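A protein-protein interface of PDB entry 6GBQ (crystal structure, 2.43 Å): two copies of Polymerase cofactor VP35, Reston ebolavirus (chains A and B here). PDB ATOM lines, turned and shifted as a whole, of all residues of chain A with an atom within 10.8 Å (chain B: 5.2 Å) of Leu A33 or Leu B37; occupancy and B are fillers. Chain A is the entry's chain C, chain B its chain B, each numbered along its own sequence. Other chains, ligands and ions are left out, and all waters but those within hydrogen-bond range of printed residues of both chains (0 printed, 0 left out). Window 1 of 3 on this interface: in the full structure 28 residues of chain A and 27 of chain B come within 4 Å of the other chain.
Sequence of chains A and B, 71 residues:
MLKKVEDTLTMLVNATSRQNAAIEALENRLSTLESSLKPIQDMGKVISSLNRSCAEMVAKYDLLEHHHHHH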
ATOM      1  N   ALA A  25      -6.444 -21.820 -40.863  1.00  0.00           N
ATOM      2  CA  ALA A  25      -7.370 -22.462 -39.923  1.00  0.00           C
ATOM      3  C   ALA A  25      -6.688 -23.677 -39.283  1.00  0.00           C
ATOM      4  O   ALA A  25      -6.789 -23.892 -38.065  1.00  0.00           O
ATOM      5  CB  ALA A  25      -8.647 -22.867 -40.623  1.00  0.00           C
ATOM      6  N   LEU A  26      -5.968 -24.436 -40.109  1.00  0.00           N
ATOM      7  CA  LEU A  26      -5.155 -25.538 -39.633  1.00  0.00           C
ATOM      8  C   LEU A  26      -4.066 -25.079 -38.653  1.00  0.00           C
ATOM      9  O   LEU A  26      -3.918 -25.673 -37.594  1.00  0.00           O
ATOM     10  CB  LEU A  26      -4.518 -26.284 -40.809  1.00  0.00           C
ATOM     11  CG  LEU A  26      -3.688 -27.515 -40.460  1.00  0.00           C
ATOM     12  CD1 LEU A  26      -4.462 -28.443 -39.531  1.00  0.00           C
ATOM     13  CD2 LEU A  26      -3.268 -28.242 -41.723  1.00  0.00           C
ATOM     14  N   GLU A  27      -3.306 -24.043 -39.014  1.00  0.00           N
ATOM     15  CA  GLU A  27      -2.304 -23.454 -38.114  1.00  0.00           C
ATOM     16  C   GLU A  27      -2.913 -23.078 -36.768  1.00  0.00           C
ATOM     17  O   GLU A  27      -2.329 -23.344 -35.720  1.00  0.00           O
ATOM     18  CB  GLU A  27      -1.663 -22.205 -38.731  1.00  0.00           C
ATOM     19  CG  GLU A  27      -0.596 -22.491 -39.773  1.00  0.00           C
ATOM     20  CD  GLU A  27      -0.212 -21.270 -40.618  1.00  0.00           C
ATOM     21  OE1 GLU A  27      -0.847 -20.190 -40.478  1.00  0.00           O
ATOM     22  OE2 GLU A  27       0.739 -21.396 -41.432  1.00  0.00           O
ATOM     23  N   ASN A  28      -4.089 -22.462 -36.814  1.00  0.00           N
ATOM     24  CA  ASN A  28      -4.770 -22.005 -35.602  1.00  0.00           C
ATOM     25  C   ASN A  28      -5.300 -23.128 -34.736  1.00  0.00           C
ATOM     26  O   ASN A  28      -5.316 -23.001 -33.506  1.00  0.00           O
ATOM     27  CB  ASN A  28      -5.897 -21.031 -35.953  1.00  0.00           C
ATOM     28  CG  ASN A  28      -5.368 -19.698 -36.468  1.00  0.00           C
ATOM     29  OD1 ASN A  28      -4.223 -19.308 -36.188  1.00  0.00           O
ATOM     30  ND2 ASN A  28      -6.191 -18.996 -37.230  1.00  0.00           N
ATOM     31  N   ARG A  29      -5.740 -24.214 -35.363  1.00  0.00           N
ATOM     32  CA  ARG A  29      -6.248 -25.341 -34.612  1.00  0.00           C
ATOM     33  C   ARG A  29      -5.090 -26.101 -33.938  1.00  0.00           C
ATOM     34  O   ARG A  29      -5.294 -26.716 -32.898  1.00  0.00           O
ATOM     35  CB  ARG A  29      -7.092 -26.265 -35.496  1.00  0.00           C
ATOM     36  CG  ARG A  29      -8.158 -27.035 -34.722  1.00  0.00           C
ATOM     37  CD  ARG A  29      -9.470 -26.274 -34.677  1.00  0.00           C
ATOM     38  NE  ARG A  29     -10.487 -26.981 -33.895  1.00  0.00           N
ATOM     39  CZ  ARG A  29     -10.599 -26.974 -32.562  1.00  0.00           C
ATOM     40  NH1 ARG A  29      -9.760 -26.283 -31.790  1.00  0.00           N
ATOM     41  NH2 ARG A  29     -11.573 -27.673 -31.981  1.00  0.00           N
ATOM     42  N   LEU A  30      -3.895 -26.063 -34.535  1.00  0.00           N
ATOM     43  CA  LEU A  30      -2.701 -26.657 -33.924  1.00  0.00           C
ATOM     44  C   LEU A  30      -2.250 -25.862 -32.685  1.00  0.00           C
ATOM     45  O   LEU A  30      -1.885 -26.451 -31.660  1.00  0.00           O
ATOM     46  CB  LEU A  30      -1.559 -26.775 -34.941  1.00  0.00           C
ATOM     47  CG  LEU A  30      -0.232 -27.394 -34.472  1.00  0.00           C
ATOM     48  CD1 LEU A  30      -0.430 -28.733 -33.770  1.00  0.00           C
ATOM     49  CD2 LEU A  30       0.769 -27.554 -35.616  1.00  0.00           C
ATOM     50  N   SER A  31      -2.269 -24.533 -32.795  1.00  0.00           N
ATOM     51  CA  SER A  31      -2.030 -23.640 -31.653  1.00  0.00           C
ATOM     52  C   SER A  31      -2.956 -23.945 -30.487  1.00  0.00           C
ATOM     53  O   SER A  31      -2.515 -24.064 -29.352  1.00  0.00           O
ATOM     54  CB  SER A  31      -2.237 -22.194 -32.073  1.00  0.00           C
ATOM     55  OG  SER A  31      -1.342 -21.868 -33.108  1.00  0.00           O
ATOM     56  N   THR A  32      -4.238 -24.094 -30.784  1.00  0.00           N
ATOM     57  CA  THR A  32      -5.221 -24.457 -29.769  1.00  0.00           C
ATOM     58  C   THR A  32      -4.900 -25.832 -29.151  1.00  0.00           C
ATOM     59  O   THR A  32      -4.965 -25.973 -27.933  1.00  0.00           O
ATOM     60  CB  THR A  32      -6.667 -24.380 -30.318  1.00  0.00           C
ATOM     61  OG1 THR A  32      -6.839 -23.141 -31.007  1.00  0.00           O
ATOM     62  CG2 THR A  32      -7.651 -24.348 -29.214  1.00  0.00           C
ATOM     63  N   LEU A  33      -4.521 -26.818 -29.973  1.00  0.00           N
ATOM     64  CA  LEU A  33      -4.086 -28.118 -29.456  1.00  0.00           C
ATOM     65  C   LEU A  33      -2.837 -28.019 -28.556  1.00  0.00           C
ATOM     66  O   LEU A  33      -2.818 -28.586 -27.461  1.00  0.00           O
ATOM     67  CB  LEU A  33      -3.824 -29.109 -30.583  1.00  0.00           C
ATOM     68  CG  LEU A  33      -3.496 -30.546 -30.143  1.00  0.00           C
ATOM     69  CD1 LEU A  33      -4.613 -31.161 -29.306  1.00  0.00           C
ATOM     70  CD2 LEU A  33      -3.204 -31.421 -31.356  1.00  0.00           C
ATOM     71  N   GLU A  34      -1.819 -27.304 -29.035  1.00  0.00           N
ATOM     72  CA  GLU A  34      -0.605 -27.051 -28.276  1.00  0.00           C
ATOM     73  C   GLU A  34      -0.937 -26.418 -26.916  1.00  0.00           C
ATOM     74  O   GLU A  34      -0.371 -26.811 -25.898  1.00  0.00           O
ATOM     75  CB  GLU A  34       0.376 -26.179 -29.087  1.00  0.00           C
ATOM     76  CG  GLU A  34       1.041 -26.925 -30.247  1.00  0.00           C
ATOM     77  CD  GLU A  34       1.801 -26.055 -31.261  1.00  0.00           C
ATOM     78  OE1 GLU A  34       1.452 -24.877 -31.486  1.00  0.00           O
ATOM     79  OE2 GLU A  34       2.758 -26.576 -31.878  1.00  0.00           O
ATOM     80  N   SER A  35      -1.875 -25.468 -26.908  1.00  0.00           N
ATOM     81  CA  SER A  35      -2.353 -24.834 -25.668  1.00  0.00           C
ATOM     82  C   SER A  35      -3.055 -25.812 -24.730  1.00  0.00           C
ATOM     83  O   SER A  35      -2.848 -25.759 -23.533  1.00  0.00           O
ATOM     84  CB  SER A  35      -3.300 -23.655 -25.965  1.00  0.00           C
ATOM     85  OG  SER A  35      -2.588 -22.543 -26.473  1.00  0.00           O
ATOM     86  N   SER A  36      -3.890 -26.686 -25.272  1.00  0.00           N
ATOM     87  CA  SER A  36      -4.611 -27.674 -24.458  1.00  0.00           C
ATOM     88  C   SER A  36      -3.703 -28.665 -23.722  1.00  0.00           C
ATOM     89  O   SER A  36      -4.098 -29.222 -22.700  1.00  0.00           O
ATOM     90  CB  SER A  36      -5.631 -28.442 -25.314  1.00  0.00           C
ATOM     91  OG  SER A  36      -6.801 -27.657 -25.506  1.00  0.00           O
ATOM     92  N   LEU A  37      -2.508 -28.903 -24.253  1.00  0.00           N
ATOM     93  CA  LEU A  37      -1.549 -29.801 -23.616  1.00  0.00           C
ATOM     94  C   LEU A  37      -0.757 -29.168 -22.485  1.00  0.00           C
ATOM     95  O   LEU A  37      -0.259 -29.901 -21.635  1.00  0.00           O
ATOM     96  CB  LEU A  37      -0.581 -30.395 -24.642  1.00  0.00           C
ATOM     97  CG  LEU A  37      -1.170 -31.518 -25.488  1.00  0.00           C
ATOM     98  CD1 LEU A  37      -0.276 -31.716 -26.702  1.00  0.00           C
ATOM     99  CD2 LEU A  37      -1.341 -32.819 -24.709  1.00  0.00           C
ATOM    100  N   LYS A  38      -0.606 -27.842 -22.477  1.00  0.00           N
ATOM    101  CA  LYS A  38       0.174 -27.162 -21.420  1.00  0.00           C
ATOM    102  C   LYS A  38      -0.284 -27.477 -19.985  1.00  0.00           C
ATOM    103  O   LYS A  38       0.539 -27.893 -19.179  1.00  0.00           O
ATOM    104  CB  LYS A  38       0.240 -25.645 -21.638  1.00  0.00           C
ATOM    105  CG  LYS A  38       1.274 -25.229 -22.672  1.00  0.00           C
ATOM    106  CD  LYS A  38       1.434 -23.712 -22.726  1.00  0.00           C
ATOM    107  CE  LYS A  38       2.337 -23.272 -23.872  1.00  0.00           C
ATOM    108  NZ  LYS A  38       1.786 -23.658 -25.207  1.00  0.00           N
ATOM    109  N   PRO A  39      -1.586 -27.301 -19.668  1.00  0.00           N
ATOM    110  CA  PRO A  39      -2.021 -27.619 -18.298  1.00  0.00           C
ATOM    111  C   PRO A  39      -1.801 -29.088 -17.899  1.00  0.00           C
ATOM    112  O   PRO A  39      -1.570 -29.364 -16.718  1.00  0.00           O
ATOM    113  CB  PRO A  39      -3.517 -27.245 -18.275  1.00  0.00           C
ATOM    114  CG  PRO A  39      -3.913 -26.984 -19.684  1.00  0.00           C
ATOM    115  CD  PRO A  39      -2.674 -26.724 -20.484  1.00  0.00           C
ATOM    116  N   ILE A  40      -1.847 -29.996 -18.877  1.00  0.00           N
ATOM    117  CA  ILE A  40      -1.547 -31.413 -18.670  1.00  0.00           C
ATOM    118  C   ILE A  40      -0.041 -31.616 -18.417  1.00  0.00           C
ATOM    119  O   ILE A  40       0.326 -32.406 -17.545  1.00  0.00           O
ATOM    120  CB  ILE A  40      -2.004 -32.293 -19.873  1.00  0.00           C
ATOM    121  CG1 ILE A  40      -3.493 -32.082 -20.175  1.00  0.00           C
ATOM    122  CG2 ILE A  40      -1.745 -33.781 -19.604  1.00  0.00           C
ATOM    123  CD1 ILE A  40      -3.993 -32.856 -21.377  1.00  0.00           C
ATOM    124  N   GLN A  41       0.818 -30.932 -19.184  1.00  0.00           N
ATOM    125  CA  GLN A  41       2.274 -30.897 -18.903  1.00  0.00           C
ATOM    126  C   GLN A  41       2.580 -30.353 -17.497  1.00  0.00           C
ATOM    127  O   GLN A  41       3.473 -30.859 -16.821  1.00  0.00           O
ATOM    128  CB  GLN A  41       3.043 -30.058 -19.944  1.00  0.00           C
ATOM    129  CG  GLN A  41       3.114 -30.664 -21.339  1.00  0.00           C
ATOM    130  CD  GLN A  41       3.624 -29.703 -22.424  1.00  0.00           C
ATOM    131  OE1 GLN A  41       3.765 -28.493 -22.207  1.00  0.00           O
ATOM    132  NE2 GLN A  41       3.894 -30.250 -23.612  1.00  0.00           N
ATOM    133  N   MET A  43       0.846 -30.697 -14.798  1.00  0.00           N
ATOM    134  CA  MET A  43       0.546 -31.718 -13.786  1.00  0.00           C
ATOM    135  C   MET A  43       1.750 -32.603 -13.428  1.00  0.00           C
ATOM    136  O   MET A  43       1.643 -33.436 -12.537  1.00  0.00           O
ATOM    137  CB  MET A  43      -0.616 -32.612 -14.240  1.00  0.00           C
ATOM    138  CG  MET A  43      -1.962 -31.911 -14.321  1.00  0.00           C
ATOM    139  SD  MET A  43      -3.254 -32.839 -15.193  1.00  0.00           S
ATOM    140  CE  MET A  43      -3.098 -34.468 -14.484  1.00  0.00           C
ATOM    141  N   LEU B  30      -7.262 -32.718 -35.767  1.00  0.00           N
ATOM    142  CA  LEU B  30      -6.767 -31.914 -34.644  1.00  0.00           C
ATOM    143  C   LEU B  30      -7.887 -31.481 -33.690  1.00  0.00           C
ATOM    144  O   LEU B  30      -7.700 -31.543 -32.479  1.00  0.00           O
ATOM    145  CB  LEU B  30      -5.967 -30.705 -35.133  1.00  0.00           C
ATOM    146  CG  LEU B  30      -4.692 -30.994 -35.954  1.00  0.00           C
ATOM    147  CD1 LEU B  30      -3.999 -29.691 -36.322  1.00  0.00           C
ATOM    148  CD2 LEU B  30      -3.708 -31.892 -35.231  1.00  0.00           C
ATOM    149  N   LEU B  33      -8.873 -34.362 -31.546  1.00  0.00           N
ATOM    150  CA  LEU B  33      -7.827 -34.586 -30.539  1.00  0.00           C
ATOM    151  C   LEU B  33      -7.920 -33.597 -29.413  1.00  0.00           C
ATOM    152  O   LEU B  33      -7.778 -33.965 -28.253  1.00  0.00           O
ATOM    153  CB  LEU B  33      -6.427 -34.528 -31.150  1.00  0.00           C
ATOM    154  CG  LEU B  33      -6.023 -35.724 -32.000  1.00  0.00           C
ATOM    155  CD1 LEU B  33      -4.657 -35.479 -32.629  1.00  0.00           C
ATOM    156  CD2 LEU B  33      -6.009 -36.989 -31.161  1.00  0.00           C
ATOM    157  N   GLU B  34      -8.173 -32.344 -29.748  1.00  0.00           N
ATOM    158  CA  GLU B  34      -8.246 -31.329 -28.725  1.00  0.00           C
ATOM    159  C   GLU B  34      -9.473 -31.538 -27.839  1.00  0.00           C
ATOM    160  O   GLU B  34      -9.340 -31.542 -26.627  1.00  0.00           O
ATOM    161  CB  GLU B  34      -8.252 -29.943 -29.328  1.00  0.00           C
ATOM    162  CG  GLU B  34      -7.916 -28.889 -28.300  1.00  0.00           C
ATOM    163  CD  GLU B  34      -8.290 -27.509 -28.770  1.00  0.00           C
ATOM    164  OE1 GLU B  34      -8.056 -27.217 -29.968  1.00  0.00           O
ATOM    165  OE2 GLU B  34      -8.822 -26.732 -27.945  1.00  0.00           O
ATOM    166  N   SER B  35     -10.644 -31.744 -28.430  1.00  0.00           N
ATOM    167  CA  SER B  35     -11.858 -31.936 -27.638  1.00  0.00           C
ATOM    168  C   SER B  35     -11.768 -33.144 -26.689  1.00  0.00           C
ATOM    169  O   SER B  35     -12.316 -33.095 -25.592  1.00  0.00           O
ATOM    170  CB  SER B  35     -13.108 -32.017 -28.522  1.00  0.00           C
ATOM    171  OG  SER B  35     -13.160 -33.231 -29.236  1.00  0.00           O
ATOM    172  N   SER B  36     -11.039 -34.190 -27.077  1.00  0.00           N
ATOM    173  CA  SER B  36     -10.834 -35.356 -26.202  1.00  0.00           C
ATOM    174  C   SER B  36      -9.942 -35.047 -24.994  1.00  0.00           C
ATOM    175  O   SER B  36     -10.066 -35.686 -23.957  1.00  0.00           O
ATOM    176  CB  SER B  36     -10.249 -36.526 -26.991  1.00  0.00           C
ATOM    177  OG  SER B  36      -8.915 -36.255 -27.390  1.00  0.00           O
ATOM    178  N   LEU B  37      -9.038 -34.079 -25.138  1.00  0.00           N
ATOM    179  CA  LEU B  37      -8.203 -33.599 -24.027  1.00  0.00           C
ATOM    180  C   LEU B  37      -8.907 -32.594 -23.090  1.00  0.00           C
ATOM    181  O   LEU B  37      -8.377 -32.270 -22.030  1.00  0.00           O
ATOM    182  CB  LEU B  37      -6.918 -32.981 -24.572  1.00  0.00           C
ATOM    183  CG  LEU B  37      -6.040 -33.928 -25.392  1.00  0.00           C
ATOM    184  CD1 LEU B  37      -4.816 -33.188 -25.897  1.00  0.00           C
ATOM    185  CD2 LEU B  37      -5.638 -35.164 -24.603  1.00  0.00           C
ATOM    186  N   LYS B  38     -10.080 -32.106 -23.485  1.00  0.00           N
ATOM    187  CA  LYS B  38     -10.857 -31.139 -22.697  1.00  0.00           C
ATOM    188  C   LYS B  38     -11.247 -31.604 -21.272  1.00  0.00           C
ATOM    189  O   LYS B  38     -11.142 -30.807 -20.341  1.00  0.00           O
ATOM    190  CB  LYS B  38     -12.105 -30.702 -23.501  1.00  0.00           C
ATOM    191  CG  LYS B  38     -12.907 -29.541 -22.934  1.00  0.00           C
ATOM    192  CD  LYS B  38     -12.127 -28.235 -22.875  1.00  0.00           C
ATOM    193  CE  LYS B  38     -12.991 -27.104 -22.334  1.00  0.00           C
ATOM    194  NZ  LYS B  38     -12.271 -26.308 -21.303  1.00  0.00           N
ATOM    195  N   PRO B  39     -11.702 -32.869 -21.095  1.00  0.00           N
ATOM    196  CA  PRO B  39     -12.034 -33.357 -19.735  1.00  0.00           C
ATOM    197  C   PRO B  39     -10.857 -33.496 -18.756  1.00  0.00           C
ATOM    198  O   PRO B  39     -11.052 -33.412 -17.537  1.00  0.00           O
ATOM    199  CB  PRO B  39     -12.679 -34.734 -19.992  1.00  0.00           C
ATOM    200  CG  PRO B  39     -12.289 -35.113 -21.372  1.00  0.00           C
ATOM    201  CD  PRO B  39     -12.178 -33.816 -22.123  1.00  0.00           C
ATOM    202  N   ILE B  40      -9.664 -33.712 -19.296  1.00  0.00           N
ATOM    203  CA  ILE B  40      -8.436 -33.874 -18.517  1.00  0.00           C
ATOM    204  C   ILE B  40      -7.883 -32.522 -18.034  1.00  0.00           C
ATOM    205  O   ILE B  40      -7.209 -32.473 -17.010  1.00  0.00           O
ATOM    206  CB  ILE B  40      -7.383 -34.671 -19.340  1.00  0.00           C
ATOM    207  CG1 ILE B  40      -7.924 -36.075 -19.665  1.00  0.00           C
ATOM    208  CG2 ILE B  40      -6.065 -34.812 -18.587  1.00  0.00           C
ATOM    209  CD1 ILE B  40      -7.305 -36.737 -20.876  1.00  0.00           C
ATOM    210  N   GLN B  41      -8.207 -31.431 -18.733  1.00  0.00           N
ATOM    211  CA  GLN B  41      -7.580 -30.108 -18.492  1.00  0.00           C
ATOM    212  C   GLN B  41      -7.706 -29.555 -17.065  1.00  0.00           C
ATOM    213  O   GLN B  41      -6.828 -28.818 -16.606  1.00  0.00           O
ATOM    214  CB  GLN B  41      -8.092 -29.055 -19.504  1.00  0.00           C
ATOM    215  CG  GLN B  41      -7.523 -29.227 -20.919  1.00  0.00           C
ATOM    216  CD  GLN B  41      -7.631 -27.984 -21.794  1.00  0.00           C
ATOM    217  OE1 GLN B  41      -8.101 -28.053 -22.933  1.00  0.00           O
ATOM    218  NE2 GLN B  41      -7.178 -26.847 -21.277  1.00  0.00           N
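The side-chain hydroxyl (OG1) of Thr A32 lies within hydrogen-bond range of the backbone carbonyl oxygen (O) of Asn A28. OG of Ser A36 sits at hydrogen-bond distance from O of Thr A32.
Among the printed residues, pairs that only touch across the chains: Thr A32 with Glu B34 (2.9 Å), Leu A26 with Leu B30 (3.5 Å), Leu A33 with Glu B34 (3.6 Å), Pro A39 with Gln B41 (3.6 Å), Leu A37 with Leu B37 (3.7 Å), Leu A33 with Leu B30 (3.9 Å), Leu A33 with Leu B37 (3.97 Å) and Ile A40 with Ile B40 (3.99 Å).
Leu A33 touches Leu B30, but with the chains exchanged Leu A30 does not touch Leu B33 (8.0 Å). Ser A36 touches Glu B34, but with the chains exchanged Glu A34 does not touch Ser B36 (11.5 Å). Ser A36 touches Gln B41, but with the chains exchanged Gln A41 does not touch Ser B36 (12.8 Å). Leu A37 touches its own counterpart, Leu B37. 10 positions are printed for both chains. Of the 11 pairs that touch across the chains among the printed residues, 2 have their exchanged pair printed and touching as well.
Printed residues of chain B within 4 Å of Leu A26: Leu B30 (3.5 Å). Printed residues of chain B within 4 Å of Arg A29: Glu B34. Leu A33 touches just these residues of chain B: Leu B30 (3.9 Å), Glu B34 (3.6 Å) and Leu B37 (3.97 Å). Printed residues of chain B within 4 Å of Ser A36: Glu B34 (3.3 Å) and Gln B41 (2.9 Å). Leu B30 touches just these residues of chain A: Leu A26 (3.5 Å) and Leu A33 (3.9 Å). No residue of chain A comes within 4 Å of Leu B33. No residue of chain A comes within 4 Å of Ser B35. Of chain A, only Leu A33 (3.97 Å) and Leu A37 (3.7 Å) come within 4 Å of Leu B37. No residue of chain A comes within 4 Å of Pro B39. Of the printed residues of chain A, Ile B40 touches Ile A40 (3.99 Å). The nearest residue of chain A that does not touch Leu B37 is Ile A40 (4.3 Å). The nearest printed residue of chain B that does not touch Leu A26 is Glu B34 (8.8 Å).
OE1 of Glu B34 lies within salt-bridge range of NH1 of Arg A29, at 2.7 Å. OG of Ser A36 lies close to OE2 of Glu B34, at 3.3 Å. OG of Ser A36 is in hydrogen-bond range of OE1 of Gln B41, at 2.9 Å.
Of the 10 printed residues of chain B, 5 touch a printed residue of chain A. Of the 18 printed residues of chain A, 8 touch a printed residue of chain B. Printed residues of chain A that touch a printed residue of chain B: Leu A26, Arg A29, Thr A32, Leu A33, Ser A36, Leu A37, Pro A39 and Ile A40. Among the printed residues, 11 pairs touch across the chains. Among the printed residues, Asp or Glu carboxylates within 4 Å of a Lys or Arg side-chain nitrogen of the other chain: Arg A29 with Glu B34 (2.7 Å).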
